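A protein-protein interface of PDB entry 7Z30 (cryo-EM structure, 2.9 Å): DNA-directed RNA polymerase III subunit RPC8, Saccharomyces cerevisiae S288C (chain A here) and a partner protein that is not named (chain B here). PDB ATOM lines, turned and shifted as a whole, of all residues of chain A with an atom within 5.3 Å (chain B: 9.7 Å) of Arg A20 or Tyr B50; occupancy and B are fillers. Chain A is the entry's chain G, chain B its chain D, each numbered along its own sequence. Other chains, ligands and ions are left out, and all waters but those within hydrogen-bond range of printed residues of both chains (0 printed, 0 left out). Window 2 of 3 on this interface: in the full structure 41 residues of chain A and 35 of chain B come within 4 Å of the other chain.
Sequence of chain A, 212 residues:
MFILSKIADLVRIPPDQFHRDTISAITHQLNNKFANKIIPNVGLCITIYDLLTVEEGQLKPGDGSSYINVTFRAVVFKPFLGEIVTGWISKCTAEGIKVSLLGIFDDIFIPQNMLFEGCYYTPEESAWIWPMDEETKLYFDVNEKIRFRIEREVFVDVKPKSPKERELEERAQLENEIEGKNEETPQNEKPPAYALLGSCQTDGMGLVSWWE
The side-chain hydroxyl of Tyr B50 sits at hydrogen-bond distance from a ring nitrogen (NE2) of His B27 (2.7 Å).
The backbone carbonyl oxygen of Lys B45 lies within hydrogen-bond range of the backbone NH of Tyr B50 (3.2 Å).
O of Ser A24 lies within hydrogen-bond range of NH2 of Arg A20.
NE2 of Gln A17 touches O of Pro B49, at 3.6 Å.
Arg B48 touches His A19.
NH1 of Arg A20 touches CD2 of Tyr B50 (3.1 Å).
Tyr B50 touches His A28.
Of the 9 printed residues of chain A, 4 touch a printed residue of chain B.
Printed residues of chain A that touch a printed residue of chain B: Gln A17, His A19, Arg A20 and His A28.
Of the 20 printed residues of chain B, 3 touch a printed residue of chain A.
Printed residues of chain B that touch a printed residue of chain A: Arg B48, Pro B49 and Tyr B50.
Hydrophobic or aromatic side chains of chain B within 4 Å of the printed part of chain A: Tyr B50.
Gln A17 touches just one residue of chain B: Pro B49 (3.6 Å).
Of chain B, only Arg B48 (3.2 Å) comes within 4 Å of His A19.
Of chain B, only Tyr B50 comes within 4 Å of Arg A20.
No residue of chain B comes within 4 Å of Asp A21.
No residue of chain B comes within 4 Å of Ala A25.
Of the printed residues of chain B, His A28 touches Tyr B50.
Of the printed residues of chain A, Arg B48 touches His A19 (3.2 Å).
Printed residues of chain A within 4 Å of Pro B49: Gln A17.
Tyr B50 touches two residues of chain A.
The nearest printed residue of chain A that does not touch Tyr B50 is Gln A17 (5.5 Å).
The nearest printed residue of chain A that does not touch Arg B48 is Gln A17 (4.5 Å).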
ATOM      1  N   GLN A  17     -16.273  27.202   9.635  1.00  0.00           N
ATOM      2  CA  GLN A  17     -16.860  27.454  10.942  1.00  0.00           C
ATOM      3  C   GLN A  17     -15.953  28.280  11.847  1.00  0.00           C
ATOM      4  O   GLN A  17     -16.174  28.321  13.061  1.00  0.00           O
ATOM      5  CB  GLN A  17     -17.217  26.132  11.622  1.00  0.00           C
ATOM      6  CG  GLN A  17     -17.520  24.999  10.660  1.00  0.00           C
ATOM      7  CD  GLN A  17     -18.927  25.064  10.094  1.00  0.00           C
ATOM      8  OE1 GLN A  17     -19.583  26.105  10.138  1.00  0.00           O
ATOM      9  NE2 GLN A  17     -19.399  23.945   9.558  1.00  0.00           N
ATOM     10  N   PHE A  18     -14.936  28.935  11.286  1.00  0.00           N
ATOM     11  CA  PHE A  18     -14.096  29.806  12.099  1.00  0.00           C
ATOM     12  C   PHE A  18     -14.809  31.096  12.476  1.00  0.00           C
ATOM     13  O   PHE A  18     -14.378  31.776  13.414  1.00  0.00           O
ATOM     14  CB  PHE A  18     -12.793  30.136  11.368  1.00  0.00           C
ATOM     15  CG  PHE A  18     -11.808  29.003  11.335  1.00  0.00           C
ATOM     16  CD1 PHE A  18     -12.069  27.817  11.999  1.00  0.00           C
ATOM     17  CD2 PHE A  18     -10.610  29.134  10.657  1.00  0.00           C
ATOM     18  CE1 PHE A  18     -11.162  26.777  11.970  1.00  0.00           C
ATOM     19  CE2 PHE A  18      -9.700  28.100  10.627  1.00  0.00           C
ATOM     20  CZ  PHE A  18      -9.975  26.921  11.285  1.00  0.00           C
ATOM     21  N   HIS A  19     -15.883  31.451  11.767  1.00  0.00           N
ATOM     22  CA  HIS A  19     -16.608  32.673  12.093  1.00  0.00           C
ATOM     23  C   HIS A  19     -17.442  32.507  13.359  1.00  0.00           C
ATOM     24  O   HIS A  19     -17.552  33.441  14.160  1.00  0.00           O
ATOM     25  CB  HIS A  19     -17.482  33.102  10.914  1.00  0.00           C
ATOM     26  CG  HIS A  19     -18.598  32.154  10.610  1.00  0.00           C
ATOM     27  ND1 HIS A  19     -18.385  30.834  10.275  1.00  0.00           N
ATOM     28  CD2 HIS A  19     -19.940  32.331  10.602  1.00  0.00           C
ATOM     29  CE1 HIS A  19     -19.545  30.243  10.063  1.00  0.00           C
ATOM     30  NE2 HIS A  19     -20.506  31.128  10.258  1.00  0.00           N
ATOM     31  N   ARG A  20     -18.038  31.334  13.555  1.00  0.00           N
ATOM     32  CA  ARG A  20     -18.766  31.081  14.789  1.00  0.00           C
ATOM     33  C   ARG A  20     -17.800  30.854  15.944  1.00  0.00           C
ATOM     34  O   ARG A  20     -16.631  30.510  15.750  1.00  0.00           O
ATOM     35  CB  ARG A  20     -19.696  29.877  14.647  1.00  0.00           C
ATOM     36  CG  ARG A  20     -20.434  29.796  13.328  1.00  0.00           C
ATOM     37  CD  ARG A  20     -20.435  28.376  12.799  1.00  0.00           C
ATOM     38  NE  ARG A  20     -20.580  27.410  13.881  1.00  0.00           N
ATOM     39  CZ  ARG A  20     -21.717  26.806  14.197  1.00  0.00           C
ATOM     40  NH1 ARG A  20     -22.836  27.056  13.539  1.00  0.00           N
ATOM     41  NH2 ARG A  20     -21.732  25.935  15.201  1.00  0.00           N
ATOM     42  N   ASP A  21     -18.304  31.054  17.157  1.00  0.00           N
ATOM     43  CA  ASP A  21     -17.473  30.913  18.344  1.00  0.00           C
ATOM     44  C   ASP A  21     -17.055  29.463  18.558  1.00  0.00           C
ATOM     45  O   ASP A  21     -17.767  28.520  18.188  1.00  0.00           O
ATOM     46  CB  ASP A  21     -18.211  31.455  19.566  1.00  0.00           C
ATOM     47  CG  ASP A  21     -19.525  30.755  19.804  1.00  0.00           C
ATOM     48  OD1 ASP A  21     -20.516  31.114  19.135  1.00  0.00           O
ATOM     49  OD2 ASP A  21     -19.573  29.847  20.654  1.00  0.00           O
ATOM     50  N   THR A  22     -15.878  29.299  19.171  1.00  0.00           N
ATOM     51  CA  THR A  22     -15.216  28.002  19.213  1.00  0.00           C
ATOM     52  C   THR A  22     -16.031  26.965  19.967  1.00  0.00           C
ATOM     53  O   THR A  22     -16.111  25.814  19.531  1.00  0.00           O
ATOM     54  CB  THR A  22     -13.832  28.141  19.846  1.00  0.00           C
ATOM     55  OG1 THR A  22     -13.217  29.353  19.393  1.00  0.00           O
ATOM     56  CG2 THR A  22     -12.954  26.962  19.459  1.00  0.00           C
ATOM     57  N   SER A  24     -19.286  26.755  20.428  1.00  0.00           N
ATOM     58  CA  SER A  24     -20.427  26.331  19.623  1.00  0.00           C
ATOM     59  C   SER A  24     -19.995  25.447  18.461  1.00  0.00           C
ATOM     60  O   SER A  24     -20.667  24.460  18.143  1.00  0.00           O
ATOM     61  CB  SER A  24     -21.205  27.545  19.119  1.00  0.00           C
ATOM     62  OG  SER A  24     -21.353  28.512  20.141  1.00  0.00           O
ATOM     63  N   ALA A  25     -18.878  25.778  17.808  1.00  0.00           N
ATOM     64  CA  ALA A  25     -18.391  24.917  16.732  1.00  0.00           C
ATOM     65  C   ALA A  25     -18.026  23.533  17.262  1.00  0.00           C
ATOM     66  O   ALA A  25     -18.340  22.507  16.640  1.00  0.00           O
ATOM     67  CB  ALA A  25     -17.196  25.569  16.039  1.00  0.00           C
ATOM     68  N   HIS A  28     -21.153  21.593  18.019  1.00  0.00           N
ATOM     69  CA  HIS A  28     -21.773  21.164  16.768  1.00  0.00           C
ATOM     70  C   HIS A  28     -21.096  19.907  16.233  1.00  0.00           C
ATOM     71  O   HIS A  28     -21.761  18.916  15.901  1.00  0.00           O
ATOM     72  CB  HIS A  28     -21.703  22.301  15.743  1.00  0.00           C
ATOM     73  CG  HIS A  28     -22.083  21.901  14.350  1.00  0.00           C
ATOM     74  ND1 HIS A  28     -21.705  22.628  13.242  1.00  0.00           N
ATOM     75  CD2 HIS A  28     -22.836  20.875  13.885  1.00  0.00           C
ATOM     76  CE1 HIS A  28     -22.186  22.054  12.154  1.00  0.00           C
ATOM     77  NE2 HIS A  28     -22.876  20.988  12.516  1.00  0.00           N
ATOM     78  N   LYS B  26     -32.494  27.104  22.730  1.00  0.00           N
ATOM     79  CA  LYS B  26     -31.256  27.676  22.215  1.00  0.00           C
ATOM     80  C   LYS B  26     -31.146  27.477  20.711  1.00  0.00           C
ATOM     81  O   LYS B  26     -30.715  28.383  19.989  1.00  0.00           O
ATOM     82  CB  LYS B  26     -30.058  27.056  22.934  1.00  0.00           C
ATOM     83  CG  LYS B  26     -28.702  27.518  22.424  1.00  0.00           C
ATOM     84  CD  LYS B  26     -27.569  26.930  23.258  1.00  0.00           C
ATOM     85  CE  LYS B  26     -26.429  27.921  23.439  1.00  0.00           C
ATOM     86  NZ  LYS B  26     -26.912  29.327  23.517  1.00  0.00           N
ATOM     87  N   HIS B  27     -31.528  26.300  20.221  1.00  0.00           N
ATOM     88  CA  HIS B  27     -31.553  26.038  18.788  1.00  0.00           C
ATOM     89  C   HIS B  27     -32.372  24.779  18.543  1.00  0.00           C
ATOM     90  O   HIS B  27     -32.784  24.091  19.481  1.00  0.00           O
ATOM     91  CB  HIS B  27     -30.139  25.906  18.215  1.00  0.00           C
ATOM     92  CG  HIS B  27     -30.026  26.355  16.792  1.00  0.00           C
ATOM     93  ND1 HIS B  27     -30.228  25.506  15.726  1.00  0.00           N
ATOM     94  CD2 HIS B  27     -29.741  27.567  16.259  1.00  0.00           C
ATOM     95  CE1 HIS B  27     -30.071  26.175  14.598  1.00  0.00           C
ATOM     96  NE2 HIS B  27     -29.771  27.427  14.893  1.00  0.00           N
ATOM     97  N   LEU B  28     -32.623  24.494  17.269  1.00  0.00           N
ATOM     98  CA  LEU B  28     -33.338  23.293  16.845  1.00  0.00           C
ATOM     99  C   LEU B  28     -34.770  23.302  17.374  1.00  0.00           C
ATOM    100  O   LEU B  28     -35.291  22.307  17.879  1.00  0.00           O
ATOM    101  CB  LEU B  28     -32.592  22.034  17.284  1.00  0.00           C
ATOM    102  CG  LEU B  28     -32.818  20.758  16.479  1.00  0.00           C
ATOM    103  CD1 LEU B  28     -32.876  21.067  14.994  1.00  0.00           C
ATOM    104  CD2 LEU B  28     -31.723  19.759  16.792  1.00  0.00           C
ATOM    105  N   TRP B  29     -35.403  24.466  17.246  1.00  0.00           N
ATOM    106  CA  TRP B  29     -36.774  24.630  17.707  1.00  0.00           C
ATOM    107  C   TRP B  29     -37.726  23.765  16.892  1.00  0.00           C
ATOM    108  O   TRP B  29     -37.635  23.695  15.664  1.00  0.00           O
ATOM    109  CB  TRP B  29     -37.195  26.094  17.617  1.00  0.00           C
ATOM    110  CG  TRP B  29     -36.260  27.051  18.300  1.00  0.00           C
ATOM    111  CD1 TRP B  29     -36.403  27.574  19.552  1.00  0.00           C
ATOM    112  CD2 TRP B  29     -35.056  27.616  17.766  1.00  0.00           C
ATOM    113  NE1 TRP B  29     -35.358  28.417  19.836  1.00  0.00           N
ATOM    114  CE2 TRP B  29     -34.517  28.461  18.755  1.00  0.00           C
ATOM    115  CE3 TRP B  29     -34.377  27.484  16.549  1.00  0.00           C
ATOM    116  CZ2 TRP B  29     -33.335  29.173  18.568  1.00  0.00           C
ATOM    117  CZ3 TRP B  29     -33.199  28.193  16.366  1.00  0.00           C
ATOM    118  CH2 TRP B  29     -32.692  29.027  17.370  1.00  0.00           C
ATOM    119  N   LYS B  32     -40.391  26.015  14.969  1.00  0.00           N
ATOM    120  CA  LYS B  32     -39.748  26.681  13.843  1.00  0.00           C
ATOM    121  C   LYS B  32     -39.416  25.709  12.718  1.00  0.00           C
ATOM    122  O   LYS B  32     -39.569  26.055  11.541  1.00  0.00           O
ATOM    123  CB  LYS B  32     -38.479  27.394  14.311  1.00  0.00           C
ATOM    124  CG  LYS B  32     -38.735  28.603  15.196  1.00  0.00           C
ATOM    125  CD  LYS B  32     -37.434  29.254  15.637  1.00  0.00           C
ATOM    126  CE  LYS B  32     -37.696  30.496  16.469  1.00  0.00           C
ATOM    127  NZ  LYS B  32     -36.433  31.125  16.937  1.00  0.00           N
ATOM    128  N   SER B  40     -33.934  29.329   2.544  1.00  0.00           N
ATOM    129  CA  SER B  40     -32.986  28.567   3.348  1.00  0.00           C
ATOM    130  C   SER B  40     -31.833  29.449   3.814  1.00  0.00           C
ATOM    131  O   SER B  40     -32.033  30.628   4.126  1.00  0.00           O
ATOM    132  N   ARG B  41     -30.621  28.891   3.859  1.00  0.00           N
ATOM    133  CA  ARG B  41     -29.483  29.644   4.376  1.00  0.00           C
ATOM    134  C   ARG B  41     -28.796  30.458   3.289  1.00  0.00           C
ATOM    135  O   ARG B  41     -28.214  31.510   3.579  1.00  0.00           O
ATOM    136  N   SER B  42     -28.844  29.994   2.044  1.00  0.00           N
ATOM    137  CA  SER B  42     -28.227  30.613   0.877  1.00  0.00           C
ATOM    138  C   SER B  42     -26.715  30.430   0.835  1.00  0.00           C
ATOM    139  O   SER B  42     -26.089  30.813  -0.163  1.00  0.00           O
ATOM    140  N   LYS B  43     -26.102  29.864   1.878  1.00  0.00           N
ATOM    141  CA  LYS B  43     -24.680  29.550   1.828  1.00  0.00           C
ATOM    142  C   LYS B  43     -24.404  28.310   0.990  1.00  0.00           C
ATOM    143  O   LYS B  43     -23.408  28.270   0.259  1.00  0.00           O
ATOM    144  N   GLY B  44     -25.270  27.302   1.077  1.00  0.00           N
ATOM    145  CA  GLY B  44     -25.119  26.094   0.292  1.00  0.00           C
ATOM    146  C   GLY B  44     -25.247  24.818   1.099  1.00  0.00           C
ATOM    147  O   GLY B  44     -25.486  23.745   0.537  1.00  0.00           O
ATOM    148  N   LYS B  45     -25.098  24.917   2.421  1.00  0.00           N
ATOM    149  CA  LYS B  45     -25.142  23.748   3.292  1.00  0.00           C
ATOM    150  C   LYS B  45     -26.088  23.948   4.470  1.00  0.00           C
ATOM    151  O   LYS B  45     -25.867  23.397   5.551  1.00  0.00           O
ATOM    152  N   GLN B  46     -27.150  24.730   4.277  1.00  0.00           N
ATOM    153  CA  GLN B  46     -28.113  24.976   5.344  1.00  0.00           C
ATOM    154  C   GLN B  46     -27.923  26.372   5.924  1.00  0.00           C
ATOM    155  O   GLN B  46     -27.043  27.118   5.481  1.00  0.00           O
ATOM    156  N   ASN B  47     -28.749  26.735   6.905  1.00  0.00           N
ATOM    157  CA  ASN B  47     -28.623  28.036   7.549  1.00  0.00           C
ATOM    158  C   ASN B  47     -27.259  28.145   8.218  1.00  0.00           C
ATOM    159  O   ASN B  47     -26.950  27.385   9.140  1.00  0.00           O
ATOM    160  N   ARG B  48     -26.454  29.095   7.749  1.00  0.00           N
ATOM    161  CA  ARG B  48     -25.072  29.259   8.186  1.00  0.00           C
ATOM    162  C   ARG B  48     -24.295  27.943   8.053  1.00  0.00           C
ATOM    163  O   ARG B  48     -23.751  27.441   9.035  1.00  0.00           O
ATOM    164  CB  ARG B  48     -25.007  29.785   9.614  1.00  0.00           C
ATOM    165  CG  ARG B  48     -23.730  30.544   9.936  1.00  0.00           C
ATOM    166  CD  ARG B  48     -23.391  31.566   8.856  1.00  0.00           C
ATOM    167  NE  ARG B  48     -24.494  32.476   8.571  1.00  0.00           N
ATOM    168  CZ  ARG B  48     -24.419  33.495   7.725  1.00  0.00           C
ATOM    169  NH1 ARG B  48     -23.307  33.761   7.060  1.00  0.00           N
ATOM    170  NH2 ARG B  48     -25.488  34.266   7.542  1.00  0.00           N
ATOM    171  N   PRO B  49     -24.168  27.418   6.819  1.00  0.00           N
ATOM    172  CA  PRO B  49     -23.715  26.037   6.593  1.00  0.00           C
ATOM    173  C   PRO B  49     -23.740  25.081   7.779  1.00  0.00           C
ATOM    174  O   PRO B  49     -22.688  24.605   8.219  1.00  0.00           O
ATOM    175  CB  PRO B  49     -22.287  26.249   6.064  1.00  0.00           C
ATOM    176  CG  PRO B  49     -22.234  27.779   5.653  1.00  0.00           C
ATOM    177  CD  PRO B  49     -23.661  28.265   5.735  1.00  0.00           C
ATOM    178  N   TYR B  50     -24.930  24.789   8.301  1.00  0.00           N
ATOM    179  CA  TYR B  50     -25.077  23.722   9.280  1.00  0.00           C
ATOM    180  C   TYR B  50     -26.481  23.142   9.196  1.00  0.00           C
ATOM    181  O   TYR B  50     -27.413  23.775   8.690  1.00  0.00           O
ATOM    182  CB  TYR B  50     -24.767  24.193  10.715  1.00  0.00           C
ATOM    183  CG  TYR B  50     -25.676  25.267  11.291  1.00  0.00           C
ATOM    184  CD1 TYR B  50     -27.000  24.998  11.620  1.00  0.00           C
ATOM    185  CD2 TYR B  50     -25.190  26.541  11.549  1.00  0.00           C
ATOM    186  CE1 TYR B  50     -27.818  25.972  12.155  1.00  0.00           C
ATOM    187  CE2 TYR B  50     -26.000  27.521  12.089  1.00  0.00           C
ATOM    188  CZ  TYR B  50     -27.313  27.232  12.388  1.00  0.00           C
ATOM    189  OH  TYR B  50     -28.122  28.207  12.924  1.00  0.00           O
ATOM    190  N   ASN B  51     -26.611  21.919   9.703  1.00  0.00           N
ATOM    191  CA  ASN B  51     -27.896  21.251   9.842  1.00  0.00           C
ATOM    192  C   ASN B  51     -27.806  20.319  11.040  1.00  0.00           C
ATOM    193  O   ASN B  51     -26.713  19.954  11.482  1.00  0.00           O
ATOM    194  CB  ASN B  51     -28.279  20.475   8.575  1.00  0.00           C
ATOM    195  CG  ASN B  51     -29.741  20.067   8.561  1.00  0.00           C
ATOM    196  OD1 ASN B  51     -30.095  18.975   9.009  1.00  0.00           O
ATOM    197  ND2 ASN B  51     -30.597  20.940   8.043  1.00  0.00           N
ATOM    198  N   HIS B  52     -28.966  19.940  11.568  1.00  0.00           N
ATOM    199  CA  HIS B  52     -29.051  19.077  12.745  1.00  0.00           C
ATOM    200  C   HIS B  52     -29.924  17.867  12.442  1.00  0.00           C
ATOM    201  O   HIS B  52     -31.093  17.809  12.841  1.00  0.00           O
ATOM    202  CB  HIS B  52     -29.590  19.847  13.949  1.00  0.00           C
ATOM    203  CG  HIS B  52     -29.061  21.242  14.061  1.00  0.00           C
ATOM    204  ND1 HIS B  52     -27.715  21.531  14.035  1.00  0.00           N
ATOM    205  CD2 HIS B  52     -29.699  22.429  14.195  1.00  0.00           C
ATOM    206  CE1 HIS B  52     -27.543  22.835  14.153  1.00  0.00           C
ATOM    207  NE2 HIS B  52     -28.732  23.404  14.249  1.00  0.00           N
ATOM    208  N   PRO B  53     -29.386  16.881  11.731  1.00  0.00           N
ATOM    209  CA  PRO B  53     -30.070  15.593  11.622  1.00  0.00           C
ATOM    210  C   PRO B  53     -29.606  14.634  12.706  1.00  0.00           C
ATOM    211  O   PRO B  53     -28.525  14.772  13.280  1.00  0.00           O
ATOM    212  CB  PRO B  53     -29.648  15.103  10.230  1.00  0.00           C
ATOM    213  CG  PRO B  53     -28.269  15.663  10.055  1.00  0.00           C
ATOM    214  CD  PRO B  53     -28.163  16.918  10.907  1.00  0.00           C
ATOM    215  N   LEU B  55     -30.172  14.415  15.566  1.00  0.00           N
ATOM    216  CA  LEU B  55     -30.170  15.016  16.896  1.00  0.00           C
ATOM    217  C   LEU B  55     -31.521  15.589  17.289  1.00  0.00           C
ATOM    218  O   LEU B  55     -31.913  15.486  18.453  1.00  0.00           O
ATOM    219  CB  LEU B  55     -29.101  16.114  16.984  1.00  0.00           C
ATOM    220  CG  LEU B  55     -29.291  17.221  18.023  1.00  0.00           C
ATOM    221  CD1 LEU B  55     -29.000  16.702  19.422  1.00  0.00           C
ATOM    222  CD2 LEU B  55     -28.407  18.413  17.703  1.00  0.00           C
